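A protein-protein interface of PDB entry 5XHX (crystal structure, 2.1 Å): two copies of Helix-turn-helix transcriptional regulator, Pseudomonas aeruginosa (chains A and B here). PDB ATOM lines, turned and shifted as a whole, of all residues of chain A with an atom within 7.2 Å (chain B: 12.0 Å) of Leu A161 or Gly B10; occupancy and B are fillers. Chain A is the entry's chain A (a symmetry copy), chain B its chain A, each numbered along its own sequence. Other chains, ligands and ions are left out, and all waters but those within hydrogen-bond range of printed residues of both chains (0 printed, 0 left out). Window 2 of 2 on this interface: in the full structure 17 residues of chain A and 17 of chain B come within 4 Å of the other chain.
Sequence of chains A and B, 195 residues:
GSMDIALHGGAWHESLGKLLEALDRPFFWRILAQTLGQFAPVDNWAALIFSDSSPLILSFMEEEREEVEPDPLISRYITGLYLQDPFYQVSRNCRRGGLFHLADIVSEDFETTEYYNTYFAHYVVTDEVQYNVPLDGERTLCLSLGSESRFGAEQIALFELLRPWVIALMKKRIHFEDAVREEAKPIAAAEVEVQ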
ATOM      1  N   LEU A  99      18.409 -23.847 -32.369  1.00  0.00           N
ATOM      2  CA  LEU A  99      17.705 -24.911 -31.666  1.00  0.00           C
ATOM      3  C   LEU A  99      16.269 -24.457 -31.489  1.00  0.00           C
ATOM      4  O   LEU A  99      16.028 -23.417 -30.879  1.00  0.00           O
ATOM      5  CB  LEU A  99      18.340 -25.205 -30.300  1.00  0.00           C
ATOM      6  CG  LEU A  99      17.586 -26.245 -29.470  1.00  0.00           C
ATOM      7  CD1 LEU A  99      17.648 -27.668 -30.122  1.00  0.00           C
ATOM      8  CD2 LEU A  99      18.142 -26.249 -28.063  1.00  0.00           C
ATOM      9  N   TYR A 131      17.590 -29.372 -34.060  1.00  0.00           N
ATOM     10  CA  TYR A 131      18.796 -28.611 -34.381  1.00  0.00           C
ATOM     11  C   TYR A 131      18.810 -28.303 -35.876  1.00  0.00           C
ATOM     12  O   TYR A 131      18.700 -29.224 -36.689  1.00  0.00           O
ATOM     13  CB  TYR A 131      20.057 -29.399 -34.023  1.00  0.00           C
ATOM     14  CG  TYR A 131      20.332 -29.580 -32.533  1.00  0.00           C
ATOM     15  CD1 TYR A 131      21.045 -28.620 -31.807  1.00  0.00           C
ATOM     16  CD2 TYR A 131      19.904 -30.720 -31.872  1.00  0.00           C
ATOM     17  CE1 TYR A 131      21.321 -28.811 -30.444  1.00  0.00           C
ATOM     18  CE2 TYR A 131      20.174 -30.924 -30.535  1.00  0.00           C
ATOM     19  CZ  TYR A 131      20.882 -29.972 -29.827  1.00  0.00           C
ATOM     20  OH  TYR A 131      21.141 -30.191 -28.506  1.00  0.00           O
ATOM     21  N   GLN A 155      15.438 -29.740 -20.068  1.00  0.00           N
ATOM     22  CA  GLN A 155      15.878 -30.415 -21.287  1.00  0.00           C
ATOM     23  C   GLN A 155      16.329 -29.413 -22.351  1.00  0.00           C
ATOM     24  O   GLN A 155      17.363 -29.616 -23.002  1.00  0.00           O
ATOM     25  CB  GLN A 155      14.758 -31.312 -21.828  1.00  0.00           C
ATOM     26  CG  GLN A 155      14.484 -32.573 -21.003  1.00  0.00           C
ATOM     27  CD  GLN A 155      13.777 -32.274 -19.692  1.00  0.00           C
ATOM     28  OE1 GLN A 155      12.850 -31.459 -19.638  1.00  0.00           O
ATOM     29  NE2 GLN A 155      14.225 -32.918 -18.624  1.00  0.00           N
ATOM     30  N   ILE A 156      15.559 -28.341 -22.562  1.00  0.00           N
ATOM     31  CA  ILE A 156      15.970 -27.319 -23.529  1.00  0.00           C
ATOM     32  C   ILE A 156      17.323 -26.734 -23.131  1.00  0.00           C
ATOM     33  O   ILE A 156      18.221 -26.563 -23.964  1.00  0.00           O
ATOM     34  CB  ILE A 156      14.910 -26.212 -23.649  1.00  0.00           C
ATOM     35  CG1 ILE A 156      13.547 -26.782 -24.067  1.00  0.00           C
ATOM     36  CG2 ILE A 156      15.384 -25.156 -24.644  1.00  0.00           C
ATOM     37  CD1 ILE A 156      13.573 -27.554 -25.350  1.00  0.00           C
ATOM     38  N   ALA A 157      17.484 -26.426 -21.842  1.00  0.00           N
ATOM     39  CA  ALA A 157      18.764 -25.939 -21.338  1.00  0.00           C
ATOM     40  C   ALA A 157      19.898 -26.899 -21.689  1.00  0.00           C
ATOM     41  O   ALA A 157      20.954 -26.483 -22.180  1.00  0.00           O
ATOM     42  CB  ALA A 157      18.669 -25.732 -19.818  1.00  0.00           C
ATOM     43  N   LEU A 158      19.690 -28.197 -21.453  1.00  0.00           N
ATOM     44  CA  LEU A 158      20.696 -29.194 -21.820  1.00  0.00           C
ATOM     45  C   LEU A 158      21.001 -29.174 -23.315  1.00  0.00           C
ATOM     46  O   LEU A 158      22.172 -29.203 -23.728  1.00  0.00           O
ATOM     47  CB  LEU A 158      20.217 -30.591 -21.411  1.00  0.00           C
ATOM     48  CG  LEU A 158      20.841 -31.168 -20.147  1.00  0.00           C
ATOM     49  CD1 LEU A 158      22.280 -31.577 -20.460  1.00  0.00           C
ATOM     50  CD2 LEU A 158      20.800 -30.149 -19.020  1.00  0.00           C
ATOM     51  N   PHE A 159      19.952 -29.191 -24.145  1.00  0.00           N
ATOM     52  CA  PHE A 159      20.156 -29.149 -25.593  1.00  0.00           C
ATOM     53  C   PHE A 159      21.012 -27.950 -25.999  1.00  0.00           C
ATOM     54  O   PHE A 159      21.854 -28.056 -26.898  1.00  0.00           O
ATOM     55  CB  PHE A 159      18.802 -29.105 -26.302  1.00  0.00           C
ATOM     56  CG  PHE A 159      18.041 -30.399 -26.258  1.00  0.00           C
ATOM     57  CD1 PHE A 159      18.687 -31.615 -26.455  1.00  0.00           C
ATOM     58  CD2 PHE A 159      16.668 -30.400 -26.031  1.00  0.00           C
ATOM     59  CE1 PHE A 159      17.967 -32.825 -26.428  1.00  0.00           C
ATOM     60  CE2 PHE A 159      15.944 -31.594 -26.002  1.00  0.00           C
ATOM     61  CZ  PHE A 159      16.598 -32.810 -26.205  1.00  0.00           C
ATOM     62  N   GLU A 160      20.815 -26.801 -25.344  1.00  0.00           N
ATOM     63  CA  GLU A 160      21.638 -25.627 -25.639  1.00  0.00           C
ATOM     64  C   GLU A 160      23.066 -25.801 -25.134  1.00  0.00           C
ATOM     65  O   GLU A 160      24.012 -25.315 -25.764  1.00  0.00           O
ATOM     66  CB  GLU A 160      21.019 -24.366 -25.007  1.00  0.00           C
ATOM     67  CG  GLU A 160      19.726 -23.849 -25.682  1.00  0.00           C
ATOM     68  CD  GLU A 160      19.981 -23.126 -27.004  1.00  0.00           C
ATOM     69  OE1 GLU A 160      21.151 -23.037 -27.453  1.00  0.00           O
ATOM     70  OE2 GLU A 160      19.003 -22.635 -27.592  1.00  0.00           O
ATOM     71  N   LEU A 161      23.242 -26.473 -23.995  1.00  0.00           N
ATOM     72  CA  LEU A 161      24.590 -26.678 -23.466  1.00  0.00           C
ATOM     73  C   LEU A 161      25.433 -27.518 -24.416  1.00  0.00           C
ATOM     74  O   LEU A 161      26.616 -27.228 -24.632  1.00  0.00           O
ATOM     75  CB  LEU A 161      24.514 -27.353 -22.091  1.00  0.00           C
ATOM     76  CG  LEU A 161      25.846 -27.399 -21.331  1.00  0.00           C
ATOM     77  CD1 LEU A 161      26.225 -26.005 -20.858  1.00  0.00           C
ATOM     78  CD2 LEU A 161      25.750 -28.353 -20.140  1.00  0.00           C
ATOM     79  N   LEU A 162      24.832 -28.567 -24.985  1.00  0.00           N
ATOM     80  CA  LEU A 162      25.531 -29.507 -25.847  1.00  0.00           C
ATOM     81  C   LEU A 162      25.608 -29.024 -27.286  1.00  0.00           C
ATOM     82  O   LEU A 162      26.427 -29.539 -28.059  1.00  0.00           O
ATOM     83  CB  LEU A 162      24.828 -30.863 -25.816  1.00  0.00           C
ATOM     84  CG  LEU A 162      24.550 -31.496 -24.453  1.00  0.00           C
ATOM     85  CD1 LEU A 162      23.984 -32.914 -24.601  1.00  0.00           C
ATOM     86  CD2 LEU A 162      25.808 -31.499 -23.622  1.00  0.00           C
ATOM     87  N   ARG A 163      24.771 -28.053 -27.638  1.00  0.00           N
ATOM     88  CA  ARG A 163      24.660 -27.567 -29.011  1.00  0.00           C
ATOM     89  C   ARG A 163      25.989 -27.274 -29.702  1.00  0.00           C
ATOM     90  O   ARG A 163      26.118 -27.635 -30.881  1.00  0.00           O
ATOM     91  CB  ARG A 163      23.761 -26.322 -28.997  1.00  0.00           C
ATOM     92  CG  ARG A 163      23.588 -25.599 -30.332  1.00  0.00           C
ATOM     93  CD  ARG A 163      22.655 -24.436 -30.069  1.00  0.00           C
ATOM     94  NE  ARG A 163      22.633 -23.480 -31.150  1.00  0.00           N
ATOM     95  CZ  ARG A 163      22.035 -22.293 -31.089  1.00  0.00           C
ATOM     96  NH1 ARG A 163      21.391 -21.919 -29.990  1.00  0.00           N
ATOM     97  NH2 ARG A 163      22.084 -21.472 -32.139  1.00  0.00           N
ATOM     98  N   PRO A 164      26.998 -26.647 -29.063  1.00  0.00           N
ATOM     99  CA  PRO A 164      28.252 -26.368 -29.791  1.00  0.00           C
ATOM    100  C   PRO A 164      28.831 -27.571 -30.521  1.00  0.00           C
ATOM    101  O   PRO A 164      29.212 -27.454 -31.694  1.00  0.00           O
ATOM    102  CB  PRO A 164      29.192 -25.869 -28.683  1.00  0.00           C
ATOM    103  CG  PRO A 164      28.298 -25.273 -27.680  1.00  0.00           C
ATOM    104  CD  PRO A 164      27.036 -26.096 -27.690  1.00  0.00           C
ATOM    105  N   TRP A 165      28.893 -28.733 -29.878  1.00  0.00           N
ATOM    106  CA  TRP A 165      29.466 -29.874 -30.568  1.00  0.00           C
ATOM    107  C   TRP A 165      28.428 -30.701 -31.313  1.00  0.00           C
ATOM    108  O   TRP A 165      28.796 -31.412 -32.253  1.00  0.00           O
ATOM    109  CB  TRP A 165      30.267 -30.767 -29.605  1.00  0.00           C
ATOM    110  CG  TRP A 165      29.531 -31.329 -28.422  1.00  0.00           C
ATOM    111  CD1 TRP A 165      29.539 -30.834 -27.154  1.00  0.00           C
ATOM    112  CD2 TRP A 165      28.718 -32.506 -28.390  1.00  0.00           C
ATOM    113  NE1 TRP A 165      28.758 -31.619 -26.334  1.00  0.00           N
ATOM    114  CE2 TRP A 165      28.258 -32.661 -27.064  1.00  0.00           C
ATOM    115  CE3 TRP A 165      28.348 -33.456 -29.348  1.00  0.00           C
ATOM    116  CZ2 TRP A 165      27.424 -33.714 -26.676  1.00  0.00           C
ATOM    117  CZ3 TRP A 165      27.520 -34.497 -28.967  1.00  0.00           C
ATOM    118  CH2 TRP A 165      27.066 -34.616 -27.639  1.00  0.00           C
ATOM    119  N   VAL A 166      27.145 -30.621 -30.941  1.00  0.00           N
ATOM    120  CA  VAL A 166      26.119 -31.274 -31.760  1.00  0.00           C
ATOM    121  C   VAL A 166      26.128 -30.698 -33.169  1.00  0.00           C
ATOM    122  O   VAL A 166      26.184 -31.434 -34.155  1.00  0.00           O
ATOM    123  CB  VAL A 166      24.728 -31.156 -31.113  1.00  0.00           C
ATOM    124  CG1 VAL A 166      23.627 -31.646 -32.105  1.00  0.00           C
ATOM    125  CG2 VAL A 166      24.688 -31.972 -29.830  1.00  0.00           C
ATOM    126  N   GLY B   9      31.536 -27.520 -15.555  1.00  0.00           N
ATOM    127  CA  GLY B   9      31.015 -27.800 -16.881  1.00  0.00           C
ATOM    128  C   GLY B   9      30.816 -26.553 -17.722  1.00  0.00           C
ATOM    129  O   GLY B   9      31.189 -25.455 -17.305  1.00  0.00           O
ATOM    130  N   GLY B  10      30.228 -26.727 -18.908  1.00  0.00           N
ATOM    131  CA  GLY B  10      29.959 -25.621 -19.812  1.00  0.00           C
ATOM    132  C   GLY B  10      31.059 -25.355 -20.824  1.00  0.00           C
ATOM    133  O   GLY B  10      30.872 -25.549 -22.035  1.00  0.00           O
ATOM    134  N   ALA B  11      32.218 -24.901 -20.332  1.00  0.00           N
ATOM    135  CA  ALA B  11      33.324 -24.556 -21.219  1.00  0.00           C
ATOM    136  C   ALA B  11      33.843 -25.771 -21.981  1.00  0.00           C
ATOM    137  O   ALA B  11      34.401 -25.622 -23.071  1.00  0.00           O
ATOM    138  CB  ALA B  11      34.461 -23.912 -20.423  1.00  0.00           C
ATOM    139  N   TRP B  12      33.678 -26.974 -21.423  1.00  0.00           N
ATOM    140  CA  TRP B  12      34.179 -28.169 -22.089  1.00  0.00           C
ATOM    141  C   TRP B  12      33.401 -28.460 -23.371  1.00  0.00           C
ATOM    142  O   TRP B  12      33.972 -28.953 -24.352  1.00  0.00           O
ATOM    143  CB  TRP B  12      34.110 -29.364 -21.143  1.00  0.00           C
ATOM    144  CG  TRP B  12      34.405 -30.659 -21.841  1.00  0.00           C
ATOM    145  CD1 TRP B  12      33.554 -31.709 -22.018  1.00  0.00           C
ATOM    146  CD2 TRP B  12      35.628 -31.017 -22.497  1.00  0.00           C
ATOM    147  NE1 TRP B  12      34.180 -32.712 -22.726  1.00  0.00           N
ATOM    148  CE2 TRP B  12      35.453 -32.310 -23.031  1.00  0.00           C
ATOM    149  CE3 TRP B  12      36.858 -30.372 -22.677  1.00  0.00           C
ATOM    150  CZ2 TRP B  12      36.457 -32.969 -23.733  1.00  0.00           C
ATOM    151  CZ3 TRP B  12      37.856 -31.030 -23.374  1.00  0.00           C
ATOM    152  CH2 TRP B  12      37.650 -32.315 -23.892  1.00  0.00           C
ATOM    153  N   HIS B  13      32.096 -28.177 -23.378  1.00  0.00           N
ATOM    154  CA  HIS B  13      31.301 -28.453 -24.571  1.00  0.00           C
ATOM    155  C   HIS B  13      31.693 -27.528 -25.709  1.00  0.00           C
ATOM    156  O   HIS B  13      31.732 -27.952 -26.870  1.00  0.00           O
ATOM    157  CB  HIS B  13      29.811 -28.338 -24.248  1.00  0.00           C
ATOM    158  CG  HIS B  13      29.326 -29.408 -23.323  1.00  0.00           C
ATOM    159  ND1 HIS B  13      28.986 -29.162 -22.009  1.00  0.00           N
ATOM    160  CD2 HIS B  13      29.180 -30.741 -23.506  1.00  0.00           C
ATOM    161  CE1 HIS B  13      28.621 -30.293 -21.430  1.00  0.00           C
ATOM    162  NE2 HIS B  13      28.729 -31.266 -22.318  1.00  0.00           N
ATOM    163  N   GLU B  14      32.010 -26.264 -25.396  1.00  0.00           N
ATOM    164  CA  GLU B  14      32.454 -25.338 -26.434  1.00  0.00           C
ATOM    165  C   GLU B  14      33.846 -25.694 -26.939  1.00  0.00           C
ATOM    166  O   GLU B  14      34.120 -25.561 -28.139  1.00  0.00           O
ATOM    167  CB  GLU B  14      32.404 -23.893 -25.922  1.00  0.00           C
ATOM    168  CG  GLU B  14      31.043 -23.246 -26.191  1.00  0.00           C
ATOM    169  CD  GLU B  14      30.886 -21.834 -25.647  1.00  0.00           C
ATOM    170  OE1 GLU B  14      31.767 -21.346 -24.902  1.00  0.00           O
ATOM    171  OE2 GLU B  14      29.857 -21.205 -25.977  1.00  0.00           O
ATOM    172  N   SER B  15      34.731 -26.164 -26.051  1.00  0.00           N
ATOM    173  CA  SER B  15      36.035 -26.655 -26.498  1.00  0.00           C
ATOM    174  C   SER B  15      35.869 -27.819 -27.455  1.00  0.00           C
ATOM    175  O   SER B  15      36.505 -27.876 -28.515  1.00  0.00           O
ATOM    176  CB  SER B  15      36.887 -27.090 -25.302  1.00  0.00           C
ATOM    177  OG  SER B  15      37.318 -25.970 -24.556  1.00  0.00           O
ATOM    178  N   LEU B  16      35.018 -28.773 -27.088  1.00  0.00           N
ATOM    179  CA  LEU B  16      34.778 -29.911 -27.964  1.00  0.00           C
ATOM    180  C   LEU B  16      34.225 -29.456 -29.312  1.00  0.00           C
ATOM    181  O   LEU B  16      34.630 -29.967 -30.363  1.00  0.00           O
ATOM    182  CB  LEU B  16      33.834 -30.889 -27.270  1.00  0.00           C
ATOM    183  CG  LEU B  16      33.495 -32.170 -28.027  1.00  0.00           C
ATOM    184  CD1 LEU B  16      34.763 -32.924 -28.445  1.00  0.00           C
ATOM    185  CD2 LEU B  16      32.585 -33.042 -27.165  1.00  0.00           C
ATOM    186  N   GLY B  17      33.310 -28.484 -29.310  1.00  0.00           N
ATOM    187  CA  GLY B  17      32.750 -28.024 -30.574  1.00  0.00           C
ATOM    188  C   GLY B  17      33.793 -27.389 -31.476  1.00  0.00           C
ATOM    189  O   GLY B  17      33.810 -27.624 -32.683  1.00  0.00           O
ATOM    190  N   LYS B  18      34.687 -26.585 -30.896  1.00  0.00           N
ATOM    191  CA  LYS B  18      35.768 -25.968 -31.663  1.00  0.00           C
ATOM    192  C   LYS B  18      36.721 -27.015 -32.241  1.00  0.00           C
ATOM    193  O   LYS B  18      37.252 -26.839 -33.340  1.00  0.00           O
ATOM    194  CB  LYS B  18      36.496 -24.973 -30.745  1.00  0.00           C
ATOM    195  CG  LYS B  18      37.885 -24.512 -31.161  1.00  0.00           C
ATOM    196  CD  LYS B  18      38.566 -23.777 -29.979  1.00  0.00           C
ATOM    197  CE  LYS B  18      39.936 -23.222 -30.355  1.00  0.00           C
ATOM    198  NZ  LYS B  18      39.968 -22.793 -31.776  1.00  0.00           N
ATOM    199  N   LEU B  19      36.932 -28.114 -31.525  1.00  0.00           N
ATOM    200  CA  LEU B  19      37.803 -29.180 -32.004  1.00  0.00           C
ATOM    201  C   LEU B  19      37.152 -29.934 -33.154  1.00  0.00           C
ATOM    202  O   LEU B  19      37.778 -30.169 -34.200  1.00  0.00           O
ATOM    203  CB  LEU B  19      38.118 -30.115 -30.840  1.00  0.00           C
ATOM    204  CG  LEU B  19      38.937 -31.364 -31.115  1.00  0.00           C
ATOM    205  CD1 LEU B  19      40.297 -30.965 -31.681  1.00  0.00           C
ATOM    206  CD2 LEU B  19      39.081 -32.138 -29.809  1.00  0.00           C
ATOM    207  N   LEU B  20      35.872 -30.293 -32.986  1.00  0.00           N
ATOM    208  CA  LEU B  20      35.139 -30.982 -34.043  1.00  0.00           C
ATOM    209  C   LEU B  20      34.979 -30.111 -35.280  1.00  0.00           C
ATOM    210  O   LEU B  20      34.971 -30.630 -36.401  1.00  0.00           O
ATOM    211  CB  LEU B  20      33.761 -31.418 -33.521  1.00  0.00           C
ATOM    212  CG  LEU B  20      33.841 -32.446 -32.395  1.00  0.00           C
ATOM    213  CD1 LEU B  20      32.460 -32.867 -31.891  1.00  0.00           C
ATOM    214  CD2 LEU B  20      34.655 -33.656 -32.878  1.00  0.00           C
ATOM    215  N   THR B  35      43.914 -28.653 -27.024  1.00  0.00           N
ATOM    216  CA  THR B  35      42.865 -29.206 -26.166  1.00  0.00           C
ATOM    217  C   THR B  35      43.456 -30.145 -25.115  1.00  0.00           C
ATOM    218  O   THR B  35      43.162 -30.025 -23.919  1.00  0.00           O
ATOM    219  CB  THR B  35      41.821 -29.938 -27.011  1.00  0.00           C
ATOM    220  OG1 THR B  35      41.374 -29.081 -28.059  1.00  0.00           O
ATOM    221  CG2 THR B  35      40.611 -30.333 -26.156  1.00  0.00           C
ATOM    222  N   GLN B  38      45.351 -28.644 -22.150  1.00  0.00           N
ATOM    223  CA  GLN B  38      44.650 -28.107 -20.990  1.00  0.00           C
ATOM    224  C   GLN B  38      44.765 -29.026 -19.786  1.00  0.00           C
ATOM    225  O   GLN B  38      44.592 -28.569 -18.652  1.00  0.00           O
ATOM    226  CB  GLN B  38      43.178 -27.858 -21.332  1.00  0.00           C
ATOM    227  CG  GLN B  38      42.982 -26.788 -22.399  1.00  0.00           C
ATOM    228  CD  GLN B  38      41.556 -26.712 -22.906  1.00  0.00           C
ATOM    229  OE1 GLN B  38      40.619 -27.144 -22.230  1.00  0.00           O
ATOM    230  NE2 GLN B  38      41.383 -26.174 -24.118  1.00  0.00           N
ATOM    231  N   PHE B  39      45.076 -30.304 -20.003  1.00  0.00           N
ATOM    232  CA  PHE B  39      45.205 -31.275 -18.923  1.00  0.00           C
ATOM    233  C   PHE B  39      46.652 -31.606 -18.576  1.00  0.00           C
ATOM    234  O   PHE B  39      46.885 -32.316 -17.593  1.00  0.00           O
ATOM    235  CB  PHE B  39      44.487 -32.588 -19.291  1.00  0.00           C
ATOM    236  CG  PHE B  39      43.092 -32.405 -19.829  1.00  0.00           C
ATOM    237  CD1 PHE B  39      41.989 -32.472 -18.981  1.00  0.00           C
ATOM    238  CD2 PHE B  39      42.875 -32.184 -21.186  1.00  0.00           C
ATOM    239  CE1 PHE B  39      40.693 -32.312 -19.476  1.00  0.00           C
ATOM    240  CE2 PHE B  39      41.585 -32.019 -21.688  1.00  0.00           C
ATOM    241  CZ  PHE B  39      40.492 -32.084 -20.833  1.00  0.00           C
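CD1 of Leu A161 touches CA of Gly B10 (3.9 Å). Leu A161 touches His B13. Leu A162 touches His B13 (CD2 to NE2, 3.2 Å). Pro A164 touches His B13 (CB to O, 3.8 Å). Glu B14 touches Pro A164 (CG to CG, 3.7 Å). Pro A164 touches Gly B17 (O to CA, 3.8 Å). CD2 of His B13 touches NE1 of Trp A165, at 3.0 Å. CG of Trp A165 touches CD2 of Leu B16 (3.7 Å). CA of Trp A165 touches CA of Gly B17, at 3.8 Å. CB of Trp A165 touches CD1 of Leu B20 (3.8 Å).
Leu A161 touches just these residues of chain B: Gly B10 (3.9 Å) and His B13 (3.4 Å). Gly B10 touches just one residue of chain A: Leu A161. No residue of chain B comes within 4 Å of Glu A160. Pro A164 touches just these residues of chain B: His B13 (3.8 Å), Glu B14 (3.7 Å) and Gly B17 (3.8 Å). Of the printed residues of chain A, His B13 touches Leu A161 (3.4 Å), Leu A162 (3.2 Å), Pro A164 (3.8 Å) and Trp A165 (3.0 Å). Of the printed residues of chain A, Glu B14 touches Pro A164 (3.7 Å). Printed residues of chain A within 4 Å of Leu B20: Trp A165 (3.8 Å). Printed residues of chain B within 4 Å of Trp A165: His B13 (3.0 Å), Leu B16 (3.7 Å), Gly B17 (3.8 Å) and Leu B20 (3.8 Å). Of the printed residues of chain A, Leu B16 touches Trp A165 (3.7 Å). Trp B12 touches none of the printed residues of chain A. The nearest residue of chain B that does not touch Leu A161 is Glu B14 (5.5 Å).
Of the 15 printed residues of chain B, 6 touch a printed residue of chain A. Printed residues of chain B that touch a printed residue of chain A: Gly B10, His B13, Glu B14, Leu B16, Gly B17 and Leu B20. Hydrophobic or aromatic side chains of chain B within 4 Å of the printed part of chain A: His B13, Leu B16 and Leu B20. Of the 14 printed residues of chain A, 4 touch a printed residue of chain B. Among the printed residues, 10 pairs touch across the chains.
No position is printed for both chains.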
